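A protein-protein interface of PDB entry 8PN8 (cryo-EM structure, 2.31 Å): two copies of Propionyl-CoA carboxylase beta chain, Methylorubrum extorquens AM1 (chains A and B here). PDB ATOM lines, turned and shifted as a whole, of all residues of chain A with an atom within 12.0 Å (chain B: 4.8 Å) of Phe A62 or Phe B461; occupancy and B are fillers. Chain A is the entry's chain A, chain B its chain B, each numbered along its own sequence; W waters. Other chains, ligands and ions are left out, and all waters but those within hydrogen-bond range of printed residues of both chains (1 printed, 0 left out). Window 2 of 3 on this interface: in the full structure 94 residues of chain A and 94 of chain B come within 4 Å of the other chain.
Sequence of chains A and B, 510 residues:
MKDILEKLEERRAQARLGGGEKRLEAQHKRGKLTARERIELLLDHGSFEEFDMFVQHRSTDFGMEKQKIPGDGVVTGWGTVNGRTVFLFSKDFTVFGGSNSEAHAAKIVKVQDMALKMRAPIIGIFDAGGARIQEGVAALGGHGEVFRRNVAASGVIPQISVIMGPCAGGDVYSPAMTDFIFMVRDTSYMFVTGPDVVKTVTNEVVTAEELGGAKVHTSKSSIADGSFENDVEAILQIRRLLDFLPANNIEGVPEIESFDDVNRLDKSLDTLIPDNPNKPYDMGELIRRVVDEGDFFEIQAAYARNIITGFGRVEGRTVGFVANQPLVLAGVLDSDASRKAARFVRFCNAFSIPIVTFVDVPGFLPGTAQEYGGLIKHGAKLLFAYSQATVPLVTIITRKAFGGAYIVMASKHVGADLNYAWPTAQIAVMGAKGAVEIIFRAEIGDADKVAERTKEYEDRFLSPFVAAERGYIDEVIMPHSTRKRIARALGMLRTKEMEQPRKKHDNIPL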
ATOM      1  N   HIS A  57      15.354   1.682 -23.890  1.00  0.00           N
ATOM      2  CA  HIS A  57      14.061   1.218 -24.365  1.00  0.00           C
ATOM      3  C   HIS A  57      13.891   1.532 -25.849  1.00  0.00           C
ATOM      4  O   HIS A  57      14.538   2.422 -26.406  1.00  0.00           O
ATOM      5  CB  HIS A  57      12.931   1.855 -23.560  1.00  0.00           C
ATOM      6  CG  HIS A  57      12.761   3.320 -23.809  1.00  0.00           C
ATOM      7  ND1 HIS A  57      12.001   3.816 -24.846  1.00  0.00           N
ATOM      8  CD2 HIS A  57      13.254   4.398 -23.156  1.00  0.00           C
ATOM      9  CE1 HIS A  57      12.034   5.135 -24.821  1.00  0.00           C
ATOM     10  NE2 HIS A  57      12.787   5.514 -23.805  1.00  0.00           N
ATOM     11  N   ARG A  58      13.000   0.778 -26.492  1.00  0.00           N
ATOM     12  CA  ARG A  58      12.708   0.941 -27.911  1.00  0.00           C
ATOM     13  C   ARG A  58      11.282   1.420 -28.159  1.00  0.00           C
ATOM     14  O   ARG A  58      10.782   1.312 -29.283  1.00  0.00           O
ATOM     15  CB  ARG A  58      12.964  -0.369 -28.657  1.00  0.00           C
ATOM     16  CG  ARG A  58      14.424  -0.782 -28.689  1.00  0.00           C
ATOM     17  CD  ARG A  58      14.589  -2.192 -29.227  1.00  0.00           C
ATOM     18  NE  ARG A  58      13.944  -3.180 -28.371  1.00  0.00           N
ATOM     19  CZ  ARG A  58      14.496  -3.707 -27.287  1.00  0.00           C
ATOM     20  NH1 ARG A  58      15.708  -3.360 -26.889  1.00  0.00           N
ATOM     21  NH2 ARG A  58      13.813  -4.607 -26.584  1.00  0.00           N
ATOM     22  N   SER A  59      10.616   1.945 -27.135  1.00  0.00           N
ATOM     23  CA  SER A  59       9.256   2.436 -27.304  1.00  0.00           C
ATOM     24  C   SER A  59       9.251   3.736 -28.098  1.00  0.00           C
ATOM     25  O   SER A  59      10.135   4.582 -27.944  1.00  0.00           O
ATOM     26  CB  SER A  59       8.597   2.648 -25.942  1.00  0.00           C
ATOM     27  OG  SER A  59       7.267   3.114 -26.089  1.00  0.00           O
ATOM     28  N   THR A  60       8.240   3.890 -28.957  1.00  0.00           N
ATOM     29  CA  THR A  60       8.102   5.077 -29.793  1.00  0.00           C
ATOM     30  C   THR A  60       6.707   5.685 -29.698  1.00  0.00           C
ATOM     31  O   THR A  60       6.324   6.480 -30.562  1.00  0.00           O
ATOM     32  CB  THR A  60       8.433   4.759 -31.254  1.00  0.00           C
ATOM     33  OG1 THR A  60       7.662   3.631 -31.687  1.00  0.00           O
ATOM     34  CG2 THR A  60       9.913   4.449 -31.415  1.00  0.00           C
ATOM     35  N   ASP A  61       5.940   5.330 -28.673  1.00  0.00           N
ATOM     36  CA  ASP A  61       4.585   5.833 -28.496  1.00  0.00           C
ATOM     37  C   ASP A  61       4.564   6.935 -27.445  1.00  0.00           C
ATOM     38  O   ASP A  61       5.305   6.884 -26.460  1.00  0.00           O
ATOM     39  CB  ASP A  61       3.631   4.710 -28.083  1.00  0.00           C
ATOM     40  CG  ASP A  61       3.403   3.701 -29.190  1.00  0.00           C
ATOM     41  OD1 ASP A  61       3.471   4.089 -30.375  1.00  0.00           O
ATOM     42  OD2 ASP A  61       3.151   2.519 -28.875  1.00  0.00           O
ATOM     43  N   PHE A  62       3.707   7.934 -27.670  1.00  0.00           N
ATOM     44  CA  PHE A  62       3.495   9.034 -26.728  1.00  0.00           C
ATOM     45  C   PHE A  62       4.794   9.780 -26.427  1.00  0.00           C
ATOM     46  O   PHE A  62       5.033  10.217 -25.300  1.00  0.00           O
ATOM     47  CB  PHE A  62       2.840   8.537 -25.438  1.00  0.00           C
ATOM     48  CG  PHE A  62       1.574   7.762 -25.663  1.00  0.00           C
ATOM     49  CD1 PHE A  62       0.390   8.415 -25.958  1.00  0.00           C
ATOM     50  CD2 PHE A  62       1.568   6.381 -25.579  1.00  0.00           C
ATOM     51  CE1 PHE A  62      -0.775   7.705 -26.167  1.00  0.00           C
ATOM     52  CE2 PHE A  62       0.405   5.666 -25.786  1.00  0.00           C
ATOM     53  CZ  PHE A  62      -0.767   6.329 -26.080  1.00  0.00           C
ATOM     54  N   GLY A  63       5.639   9.929 -27.444  1.00  0.00           N
ATOM     55  CA  GLY A  63       6.854  10.702 -27.295  1.00  0.00           C
ATOM     56  C   GLY A  63       7.902  10.094 -26.394  1.00  0.00           C
ATOM     57  O   GLY A  63       8.726  10.825 -25.839  1.00  0.00           O
ATOM     58  N   MET A  64       7.897   8.770 -26.225  1.00  0.00           N
ATOM     59  CA  MET A  64       8.899   8.127 -25.384  1.00  0.00           C
ATOM     60  C   MET A  64      10.277   8.114 -26.028  1.00  0.00           C
ATOM     61  O   MET A  64      11.279   8.033 -25.311  1.00  0.00           O
ATOM     62  CB  MET A  64       8.470   6.698 -25.050  1.00  0.00           C
ATOM     63  CG  MET A  64       7.348   6.612 -24.032  1.00  0.00           C
ATOM     64  SD  MET A  64       7.829   7.219 -22.405  1.00  0.00           S
ATOM     65  CE  MET A  64       9.108   6.044 -21.973  1.00  0.00           C
ATOM     66  N   GLU A  65      10.353   8.199 -27.358  1.00  0.00           N
ATOM     67  CA  GLU A  65      11.642   8.150 -28.039  1.00  0.00           C
ATOM     68  C   GLU A  65      12.509   9.364 -27.734  1.00  0.00           C
ATOM     69  O   GLU A  65      13.718   9.323 -27.982  1.00  0.00           O
ATOM     70  CB  GLU A  65      11.440   8.022 -29.550  1.00  0.00           C
ATOM     71  CG  GLU A  65      10.884   9.268 -30.226  1.00  0.00           C
ATOM     72  CD  GLU A  65       9.401   9.464 -29.981  1.00  0.00           C
ATOM     73  OE1 GLU A  65       8.741   8.512 -29.517  1.00  0.00           O
ATOM     74  OE2 GLU A  65       8.896  10.574 -30.252  1.00  0.00           O
ATOM     75  N   LYS A  66      11.926  10.441 -27.207  1.00  0.00           N
ATOM     76  CA  LYS A  66      12.704  11.610 -26.825  1.00  0.00           C
ATOM     77  C   LYS A  66      13.356  11.468 -25.456  1.00  0.00           C
ATOM     78  O   LYS A  66      14.144  12.338 -25.071  1.00  0.00           O
ATOM     79  CB  LYS A  66      11.824  12.863 -26.841  1.00  0.00           C
ATOM     80  CG  LYS A  66      11.357  13.274 -28.225  1.00  0.00           C
ATOM     81  CD  LYS A  66      10.657  14.622 -28.191  1.00  0.00           C
ATOM     82  CE  LYS A  66       9.392  14.567 -27.351  1.00  0.00           C
ATOM     83  NZ  LYS A  66       8.378  13.659 -27.948  1.00  0.00           N
ATOM     84  N   GLN A  67      13.051  10.402 -24.718  1.00  0.00           N
ATOM     85  CA  GLN A  67      13.620  10.156 -23.392  1.00  0.00           C
ATOM     86  C   GLN A  67      14.228   8.757 -23.399  1.00  0.00           C
ATOM     87  O   GLN A  67      13.540   7.770 -23.128  1.00  0.00           O
ATOM     88  CB  GLN A  67      12.564  10.305 -22.304  1.00  0.00           C
ATOM     89  CG  GLN A  67      11.872  11.655 -22.292  1.00  0.00           C
ATOM     90  CD  GLN A  67      10.858  11.778 -21.178  1.00  0.00           C
ATOM     91  OE1 GLN A  67      10.844  10.976 -20.245  1.00  0.00           O
ATOM     92  NE2 GLN A  67       9.998  12.786 -21.269  1.00  0.00           N
ATOM     93  N   LYS A  68      15.517   8.673 -23.710  1.00  0.00           N
ATOM     94  CA  LYS A  68      16.254   7.412 -23.707  1.00  0.00           C
ATOM     95  C   LYS A  68      17.327   7.501 -22.627  1.00  0.00           C
ATOM     96  O   LYS A  68      18.378   8.114 -22.833  1.00  0.00           O
ATOM     97  CB  LYS A  68      16.857   7.121 -25.078  1.00  0.00           C
ATOM     98  CG  LYS A  68      15.827   6.911 -26.175  1.00  0.00           C
ATOM     99  CD  LYS A  68      16.487   6.520 -27.486  1.00  0.00           C
ATOM    100  CE  LYS A  68      15.462   6.367 -28.597  1.00  0.00           C
ATOM    101  NZ  LYS A  68      14.420   5.362 -28.254  1.00  0.00           N
ATOM    102  N   PHE A  96      12.352   6.953 -15.002  1.00  0.00           N
ATOM    103  CA  PHE A  96      10.961   6.627 -15.326  1.00  0.00           C
ATOM    104  C   PHE A  96      10.203   6.102 -14.111  1.00  0.00           C
ATOM    105  O   PHE A  96       9.257   5.323 -14.246  1.00  0.00           O
ATOM    106  CB  PHE A  96      10.873   5.623 -16.481  1.00  0.00           C
ATOM    107  CG  PHE A  96      11.486   6.113 -17.760  1.00  0.00           C
ATOM    108  CD1 PHE A  96      10.868   7.103 -18.505  1.00  0.00           C
ATOM    109  CD2 PHE A  96      12.674   5.576 -18.223  1.00  0.00           C
ATOM    110  CE1 PHE A  96      11.430   7.553 -19.682  1.00  0.00           C
ATOM    111  CE2 PHE A  96      13.240   6.023 -19.400  1.00  0.00           C
ATOM    112  CZ  PHE A  96      12.616   7.011 -20.131  1.00  0.00           C
ATOM    113  N   ALA A 131       4.286  -0.864 -13.837  1.00  0.00           N
ATOM    114  CA  ALA A 131       4.648  -1.032 -15.235  1.00  0.00           C
ATOM    115  C   ALA A 131       4.419   0.265 -16.000  1.00  0.00           C
ATOM    116  O   ALA A 131       3.525   1.051 -15.672  1.00  0.00           O
ATOM    117  CB  ALA A 131       3.846  -2.165 -15.882  1.00  0.00           C
ATOM    118  N   ARG A 132       5.241   0.480 -17.025  1.00  0.00           N
ATOM    119  CA  ARG A 132       5.190   1.715 -17.798  1.00  0.00           C
ATOM    120  C   ARG A 132       3.946   1.728 -18.679  1.00  0.00           C
ATOM    121  O   ARG A 132       3.729   0.806 -19.472  1.00  0.00           O
ATOM    122  CB  ARG A 132       6.453   1.849 -18.641  1.00  0.00           C
ATOM    123  CG  ARG A 132       6.838   3.272 -18.989  1.00  0.00           C
ATOM    124  CD  ARG A 132       8.274   3.322 -19.468  1.00  0.00           C
ATOM    125  NE  ARG A 132       9.189   2.760 -18.483  1.00  0.00           N
ATOM    126  CZ  ARG A 132      10.483   2.560 -18.690  1.00  0.00           C
ATOM    127  NH1 ARG A 132      11.052   2.859 -19.847  1.00  0.00           N
ATOM    128  NH2 ARG A 132      11.224   2.043 -17.715  1.00  0.00           N
ATOM    129  N   ILE A 133       3.129   2.774 -18.540  1.00  0.00           N
ATOM    130  CA  ILE A 133       1.854   2.823 -19.251  1.00  0.00           C
ATOM    131  C   ILE A 133       2.076   3.020 -20.746  1.00  0.00           C
ATOM    132  O   ILE A 133       1.378   2.422 -21.573  1.00  0.00           O
ATOM    133  CB  ILE A 133       0.956   3.924 -18.660  1.00  0.00           C
ATOM    134  CG1 ILE A 133       0.752   3.695 -17.164  1.00  0.00           C
ATOM    135  CG2 ILE A 133      -0.388   3.952 -19.367  1.00  0.00           C
ATOM    136  CD1 ILE A 133       0.099   2.374 -16.838  1.00  0.00           C
ATOM    137  N   GLN A 134       3.042   3.860 -21.118  1.00  0.00           N
ATOM    138  CA  GLN A 134       3.294   4.134 -22.528  1.00  0.00           C
ATOM    139  C   GLN A 134       3.821   2.918 -23.277  1.00  0.00           C
ATOM    140  O   GLN A 134       3.658   2.843 -24.499  1.00  0.00           O
ATOM    141  CB  GLN A 134       4.280   5.294 -22.676  1.00  0.00           C
ATOM    142  CG  GLN A 134       3.766   6.638 -22.181  1.00  0.00           C
ATOM    143  CD  GLN A 134       3.898   6.805 -20.680  1.00  0.00           C
ATOM    144  OE1 GLN A 134       4.351   5.901 -19.979  1.00  0.00           O
ATOM    145  NE2 GLN A 134       3.505   7.970 -20.179  1.00  0.00           N
ATOM    146  N   GLU A 135       4.448   1.968 -22.580  1.00  0.00           N
ATOM    147  CA  GLU A 135       4.983   0.789 -23.254  1.00  0.00           C
ATOM    148  C   GLU A 135       3.876  -0.146 -23.724  1.00  0.00           C
ATOM    149  O   GLU A 135       4.039  -0.831 -24.740  1.00  0.00           O
ATOM    150  CB  GLU A 135       5.944   0.048 -22.328  1.00  0.00           C
ATOM    151  CG  GLU A 135       7.214   0.813 -22.005  1.00  0.00           C
ATOM    152  CD  GLU A 135       8.375   0.420 -22.893  1.00  0.00           C
ATOM    153  OE1 GLU A 135       8.316  -0.667 -23.504  1.00  0.00           O
ATOM    154  OE2 GLU A 135       9.348   1.197 -22.977  1.00  0.00           O
ATOM    155  N   GLY A 136       2.757  -0.194 -23.008  1.00  0.00           N
ATOM    156  CA  GLY A 136       1.659  -1.054 -23.397  1.00  0.00           C
ATOM    157  C   GLY A 136       1.813  -2.488 -22.934  1.00  0.00           C
ATOM    158  O   GLY A 136       2.345  -2.748 -21.852  1.00  0.00           O
ATOM    159  N   VAL A 137       1.350  -3.431 -23.759  1.00  0.00           N
ATOM    160  CA  VAL A 137       1.335  -4.840 -23.384  1.00  0.00           C
ATOM    161  C   VAL A 137       2.720  -5.472 -23.394  1.00  0.00           C
ATOM    162  O   VAL A 137       2.892  -6.582 -22.873  1.00  0.00           O
ATOM    163  CB  VAL A 137       0.369  -5.601 -24.317  1.00  0.00           C
ATOM    164  CG1 VAL A 137       1.017  -5.861 -25.669  1.00  0.00           C
ATOM    165  CG2 VAL A 137      -0.113  -6.894 -23.671  1.00  0.00           C
ATOM    166  N   ALA A 138       3.719  -4.794 -23.965  1.00  0.00           N
ATOM    167  CA  ALA A 138       5.083  -5.316 -23.925  1.00  0.00           C
ATOM    168  C   ALA A 138       5.610  -5.378 -22.496  1.00  0.00           C
ATOM    169  O   ALA A 138       6.307  -6.331 -22.121  1.00  0.00           O
ATOM    170  CB  ALA A 138       5.995  -4.458 -24.800  1.00  0.00           C
ATOM    171  N   ALA A 139       5.291  -4.367 -21.685  1.00  0.00           N
ATOM    172  CA  ALA A 139       5.677  -4.400 -20.280  1.00  0.00           C
ATOM    173  C   ALA A 139       5.007  -5.559 -19.554  1.00  0.00           C
ATOM    174  O   ALA A 139       5.625  -6.211 -18.705  1.00  0.00           O
ATOM    175  CB  ALA A 139       5.332  -3.070 -19.611  1.00  0.00           C
ATOM    176  N   LEU A 140       3.741  -5.832 -19.878  1.00  0.00           N
ATOM    177  CA  LEU A 140       3.056  -6.978 -19.289  1.00  0.00           C
ATOM    178  C   LEU A 140       3.723  -8.288 -19.692  1.00  0.00           C
ATOM    179  O   LEU A 140       3.863  -9.202 -18.872  1.00  0.00           O
ATOM    180  CB  LEU A 140       1.587  -6.977 -19.705  1.00  0.00           C
ATOM    181  CG  LEU A 140       0.801  -5.700 -19.416  1.00  0.00           C
ATOM    182  CD1 LEU A 140      -0.623  -5.833 -19.923  1.00  0.00           C
ATOM    183  CD2 LEU A 140       0.821  -5.382 -17.930  1.00  0.00           C
ATOM    184  N   ILE B 427      -7.050  -6.456 -24.839  1.00  0.00           N
ATOM    185  CA  ILE B 427      -5.814  -6.745 -24.123  1.00  0.00           C
ATOM    186  C   ILE B 427      -5.036  -5.442 -24.010  1.00  0.00           C
ATOM    187  O   ILE B 427      -4.520  -4.927 -25.009  1.00  0.00           O
ATOM    188  CB  ILE B 427      -4.993  -7.829 -24.831  1.00  0.00           C
ATOM    189  CG1 ILE B 427      -5.890  -9.013 -25.192  1.00  0.00           C
ATOM    190  CG2 ILE B 427      -3.842  -8.284 -23.953  1.00  0.00           C
ATOM    191  CD1 ILE B 427      -5.216 -10.053 -26.043  1.00  0.00           C
ATOM    192  N   ALA B 428      -4.944  -4.911 -22.795  1.00  0.00           N
ATOM    193  CA  ALA B 428      -4.280  -3.638 -22.560  1.00  0.00           C
ATOM    194  C   ALA B 428      -3.822  -3.590 -21.111  1.00  0.00           C
ATOM    195  O   ALA B 428      -4.154  -4.461 -20.306  1.00  0.00           O
ATOM    196  CB  ALA B 428      -5.201  -2.459 -22.885  1.00  0.00           C
ATOM    197  N   ILE B 439      -1.356   9.055 -18.739  1.00  0.00           N
ATOM    198  CA  ILE B 439      -0.449   9.543 -19.775  1.00  0.00           C
ATOM    199  C   ILE B 439      -0.586  11.051 -19.936  1.00  0.00           C
ATOM    200  O   ILE B 439       0.382  11.802 -19.771  1.00  0.00           O
ATOM    201  CB  ILE B 439      -0.705   8.811 -21.104  1.00  0.00           C
ATOM    202  CG1 ILE B 439      -0.342   7.330 -20.976  1.00  0.00           C
ATOM    203  CG2 ILE B 439       0.082   9.458 -22.230  1.00  0.00           C
ATOM    204  CD1 ILE B 439      -0.642   6.520 -22.213  1.00  0.00           C
ATOM    205  N   PHE B 440      -1.790  11.516 -20.261  1.00  0.00           N
ATOM    206  CA  PHE B 440      -2.037  12.942 -20.466  1.00  0.00           C
ATOM    207  C   PHE B 440      -2.536  13.583 -19.171  1.00  0.00           C
ATOM    208  O   PHE B 440      -3.627  14.146 -19.089  1.00  0.00           O
ATOM    209  CB  PHE B 440      -3.023  13.148 -21.609  1.00  0.00           C
ATOM    210  CG  PHE B 440      -2.604  12.493 -22.891  1.00  0.00           C
ATOM    211  CD1 PHE B 440      -1.684  13.103 -23.726  1.00  0.00           C
ATOM    212  CD2 PHE B 440      -3.132  11.270 -23.265  1.00  0.00           C
ATOM    213  CE1 PHE B 440      -1.296  12.503 -24.906  1.00  0.00           C
ATOM    214  CE2 PHE B 440      -2.750  10.666 -24.445  1.00  0.00           C
ATOM    215  CZ  PHE B 440      -1.831  11.284 -25.266  1.00  0.00           C
ATOM    216  N   TYR B 457      -7.259   6.337 -27.924  1.00  0.00           N
ATOM    217  CA  TYR B 457      -6.659   5.224 -27.197  1.00  0.00           C
ATOM    218  C   TYR B 457      -7.530   3.977 -27.281  1.00  0.00           C
ATOM    219  O   TYR B 457      -7.019   2.861 -27.429  1.00  0.00           O
ATOM    220  CB  TYR B 457      -6.420   5.613 -25.739  1.00  0.00           C
ATOM    221  CG  TYR B 457      -5.469   4.690 -25.013  1.00  0.00           C
ATOM    222  CD1 TYR B 457      -5.920   3.518 -24.421  1.00  0.00           C
ATOM    223  CD2 TYR B 457      -4.117   4.990 -24.923  1.00  0.00           C
ATOM    224  CE1 TYR B 457      -5.054   2.673 -23.764  1.00  0.00           C
ATOM    225  CE2 TYR B 457      -3.243   4.151 -24.264  1.00  0.00           C
ATOM    226  CZ  TYR B 457      -3.716   2.994 -23.687  1.00  0.00           C
ATOM    227  OH  TYR B 457      -2.847   2.155 -23.031  1.00  0.00           O
ATOM    228  N   GLU B 458      -8.850   4.148 -27.179  1.00  0.00           N
ATOM    229  CA  GLU B 458      -9.762   3.015 -27.295  1.00  0.00           C
ATOM    230  C   GLU B 458      -9.653   2.357 -28.663  1.00  0.00           C
ATOM    231  O   GLU B 458      -9.599   1.126 -28.766  1.00  0.00           O
ATOM    232  CB  GLU B 458     -11.196   3.479 -27.038  1.00  0.00           C
ATOM    233  CG  GLU B 458     -12.259   2.463 -27.411  1.00  0.00           C
ATOM    234  CD  GLU B 458     -12.353   1.327 -26.418  1.00  0.00           C
ATOM    235  OE1 GLU B 458     -12.124   1.571 -25.216  1.00  0.00           O
ATOM    236  OE2 GLU B 458     -12.655   0.190 -26.839  1.00  0.00           O
ATOM    237  N   ASP B 459      -9.614   3.161 -29.725  1.00  0.00           N
ATOM    238  CA  ASP B 459      -9.536   2.596 -31.068  1.00  0.00           C
ATOM    239  C   ASP B 459      -8.170   1.988 -31.352  1.00  0.00           C
ATOM    240  O   ASP B 459      -8.061   1.075 -32.177  1.00  0.00           O
ATOM    241  CB  ASP B 459      -9.864   3.666 -32.109  1.00  0.00           C
ATOM    242  CG  ASP B 459     -11.271   4.208 -31.963  1.00  0.00           C
ATOM    243  OD1 ASP B 459     -12.143   3.476 -31.448  1.00  0.00           O
ATOM    244  OD2 ASP B 459     -11.508   5.366 -32.365  1.00  0.00           O
ATOM    245  N   ARG B 460      -7.123   2.470 -30.685  1.00  0.00           N
ATOM    246  CA  ARG B 460      -5.772   2.038 -31.016  1.00  0.00           C
ATOM    247  C   ARG B 460      -5.276   0.871 -30.172  1.00  0.00           C
ATOM    248  O   ARG B 460      -4.488   0.058 -30.669  1.00  0.00           O
ATOM    249  CB  ARG B 460      -4.806   3.218 -30.871  1.00  0.00           C
ATOM    250  CG  ARG B 460      -3.406   2.954 -31.385  1.00  0.00           C
ATOM    251  CD  ARG B 460      -2.528   4.179 -31.214  1.00  0.00           C
ATOM    252  NE  ARG B 460      -1.143   3.912 -31.579  1.00  0.00           N
ATOM    253  CZ  ARG B 460      -0.133   4.735 -31.331  1.00  0.00           C
ATOM    254  NH1 ARG B 460      -0.317   5.885 -30.706  1.00  0.00           N
ATOM    255  NH2 ARG B 460       1.092   4.391 -31.717  1.00  0.00           N
ATOM    256  N   PHE B 461      -5.713   0.750 -28.921  1.00  0.00           N
ATOM    257  CA  PHE B 461      -5.105  -0.208 -28.007  1.00  0.00           C
ATOM    258  C   PHE B 461      -6.068  -1.215 -27.400  1.00  0.00           C
ATOM    259  O   PHE B 461      -5.640  -2.325 -27.078  1.00  0.00           O
ATOM    260  CB  PHE B 461      -4.381   0.526 -26.870  1.00  0.00           C
ATOM    261  CG  PHE B 461      -3.202   1.331 -27.328  1.00  0.00           C
ATOM    262  CD1 PHE B 461      -2.025   0.707 -27.697  1.00  0.00           C
ATOM    263  CD2 PHE B 461      -3.270   2.711 -27.390  1.00  0.00           C
ATOM    264  CE1 PHE B 461      -0.938   1.442 -28.120  1.00  0.00           C
ATOM    265  CE2 PHE B 461      -2.186   3.451 -27.810  1.00  0.00           C
ATOM    266  CZ  PHE B 461      -1.019   2.817 -28.176  1.00  0.00           C
ATOM    267  N   LEU B 462      -7.344  -0.873 -27.225  1.00  0.00           N
ATOM    268  CA  LEU B 462      -8.300  -1.804 -26.623  1.00  0.00           C
ATOM    269  C   LEU B 462      -8.854  -2.729 -27.707  1.00  0.00           C
ATOM    270  O   LEU B 462     -10.024  -2.685 -28.089  1.00  0.00           O
ATOM    271  CB  LEU B 462      -9.401  -1.054 -25.889  1.00  0.00           C
ATOM    272  CG  LEU B 462      -9.062  -0.739 -24.430  1.00  0.00           C
ATOM    273  CD1 LEU B 462      -8.140   0.466 -24.325  1.00  0.00           C
ATOM    274  CD2 LEU B 462     -10.317  -0.539 -23.601  1.00  0.00           C
ATOM    275  N   SER B 463      -7.970  -3.590 -28.198  1.00  0.00           N
ATOM    276  CA  SER B 463      -8.270  -4.533 -29.262  1.00  0.00           C
ATOM    277  C   SER B 463      -7.323  -5.713 -29.119  1.00  0.00           C
ATOM    278  O   SER B 463      -6.285  -5.600 -28.457  1.00  0.00           O
ATOM    279  CB  SER B 463      -8.119  -3.881 -30.643  1.00  0.00           C
ATOM    280  OG  SER B 463      -6.796  -3.420 -30.848  1.00  0.00           O
ATOM    281  N   VAL B 466      -3.023  -5.428 -30.940  1.00  0.00           N
ATOM    282  CA  VAL B 466      -1.725  -4.989 -30.439  1.00  0.00           C
ATOM    283  C   VAL B 466      -0.944  -6.174 -29.886  1.00  0.00           C
ATOM    284  O   VAL B 466       0.268  -6.291 -30.098  1.00  0.00           O
ATOM    285  CB  VAL B 466      -1.899  -3.877 -29.390  1.00  0.00           C
ATOM    286  CG1 VAL B 466      -0.548  -3.448 -28.845  1.00  0.00           C
ATOM    287  CG2 VAL B 466      -2.627  -2.692 -29.994  1.00  0.00           C
HETATM  288  O   HOH W   1      -0.549   2.193 -23.754  1.00  0.00           O
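Among the printed residues, merely in contact across the chains: Phe A62 with Ile B439 (3.8 Å), Phe A62 with Phe B440 (3.7 Å), Phe A62 with Tyr B457 (3.8 Å), Phe A62 with Phe B461 (3.6 Å), Ile A133 with Ile B439 (3.7 Å), Gln A134 with Ile B439 (3.98 Å), Val A137 with Ile B427 (3.99 Å) and Leu A140 with Ala B428 (3.8 Å).
Of the printed residues of chain B, Asp A61 touches Arg B460 (2.7 Å).
Phe A62 touches just these residues of chain B: Ile B439 (3.8 Å), Phe B440 (3.7 Å), Tyr B457 (3.8 Å) and Phe B461 (3.6 Å).
Phe A96 touches none of the printed residues of chain B.
Printed residues of chain B within 4 Å of Ile A133: Ile B439 (3.7 Å).
Printed residues of chain B within 4 Å of Val A137: Ile B427.
Ala B428 touches just one residue of chain A: Leu A140 (3.8 Å).
Of the printed residues of chain A, Tyr B457 touches Phe A62.
No residue of chain A comes within 4 Å of Glu B458.
Of the printed residues of chain A, Arg B460 touches Asp A61 (2.7 Å).
Phe B461 touches just one residue of chain A: Phe A62 (3.6 Å).
No residue of chain A comes within 4 Å of Ser B463.
No residue of chain A comes within 4 Å of Val B466.
The nearest residue of chain A that does not touch Phe B461 is Asp A61 (4.2 Å).
Among the printed residues, Asp or Glu carboxylates within 4 Å of a Lys or Arg side-chain nitrogen of the other chain: Asp A61 with Arg B460 (2.7 Å).
No position is printed for both chains.
OD1 of Asp A61 lies within salt-bridge range of NH2 of Arg B460 (2.7 Å).
Water W1 lies within hydrogen-bond range of the side-chain hydroxyl of Tyr B457 (2.4 Å) and the backbone carbonyl oxygen of Ile A133 (2.9 Å).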
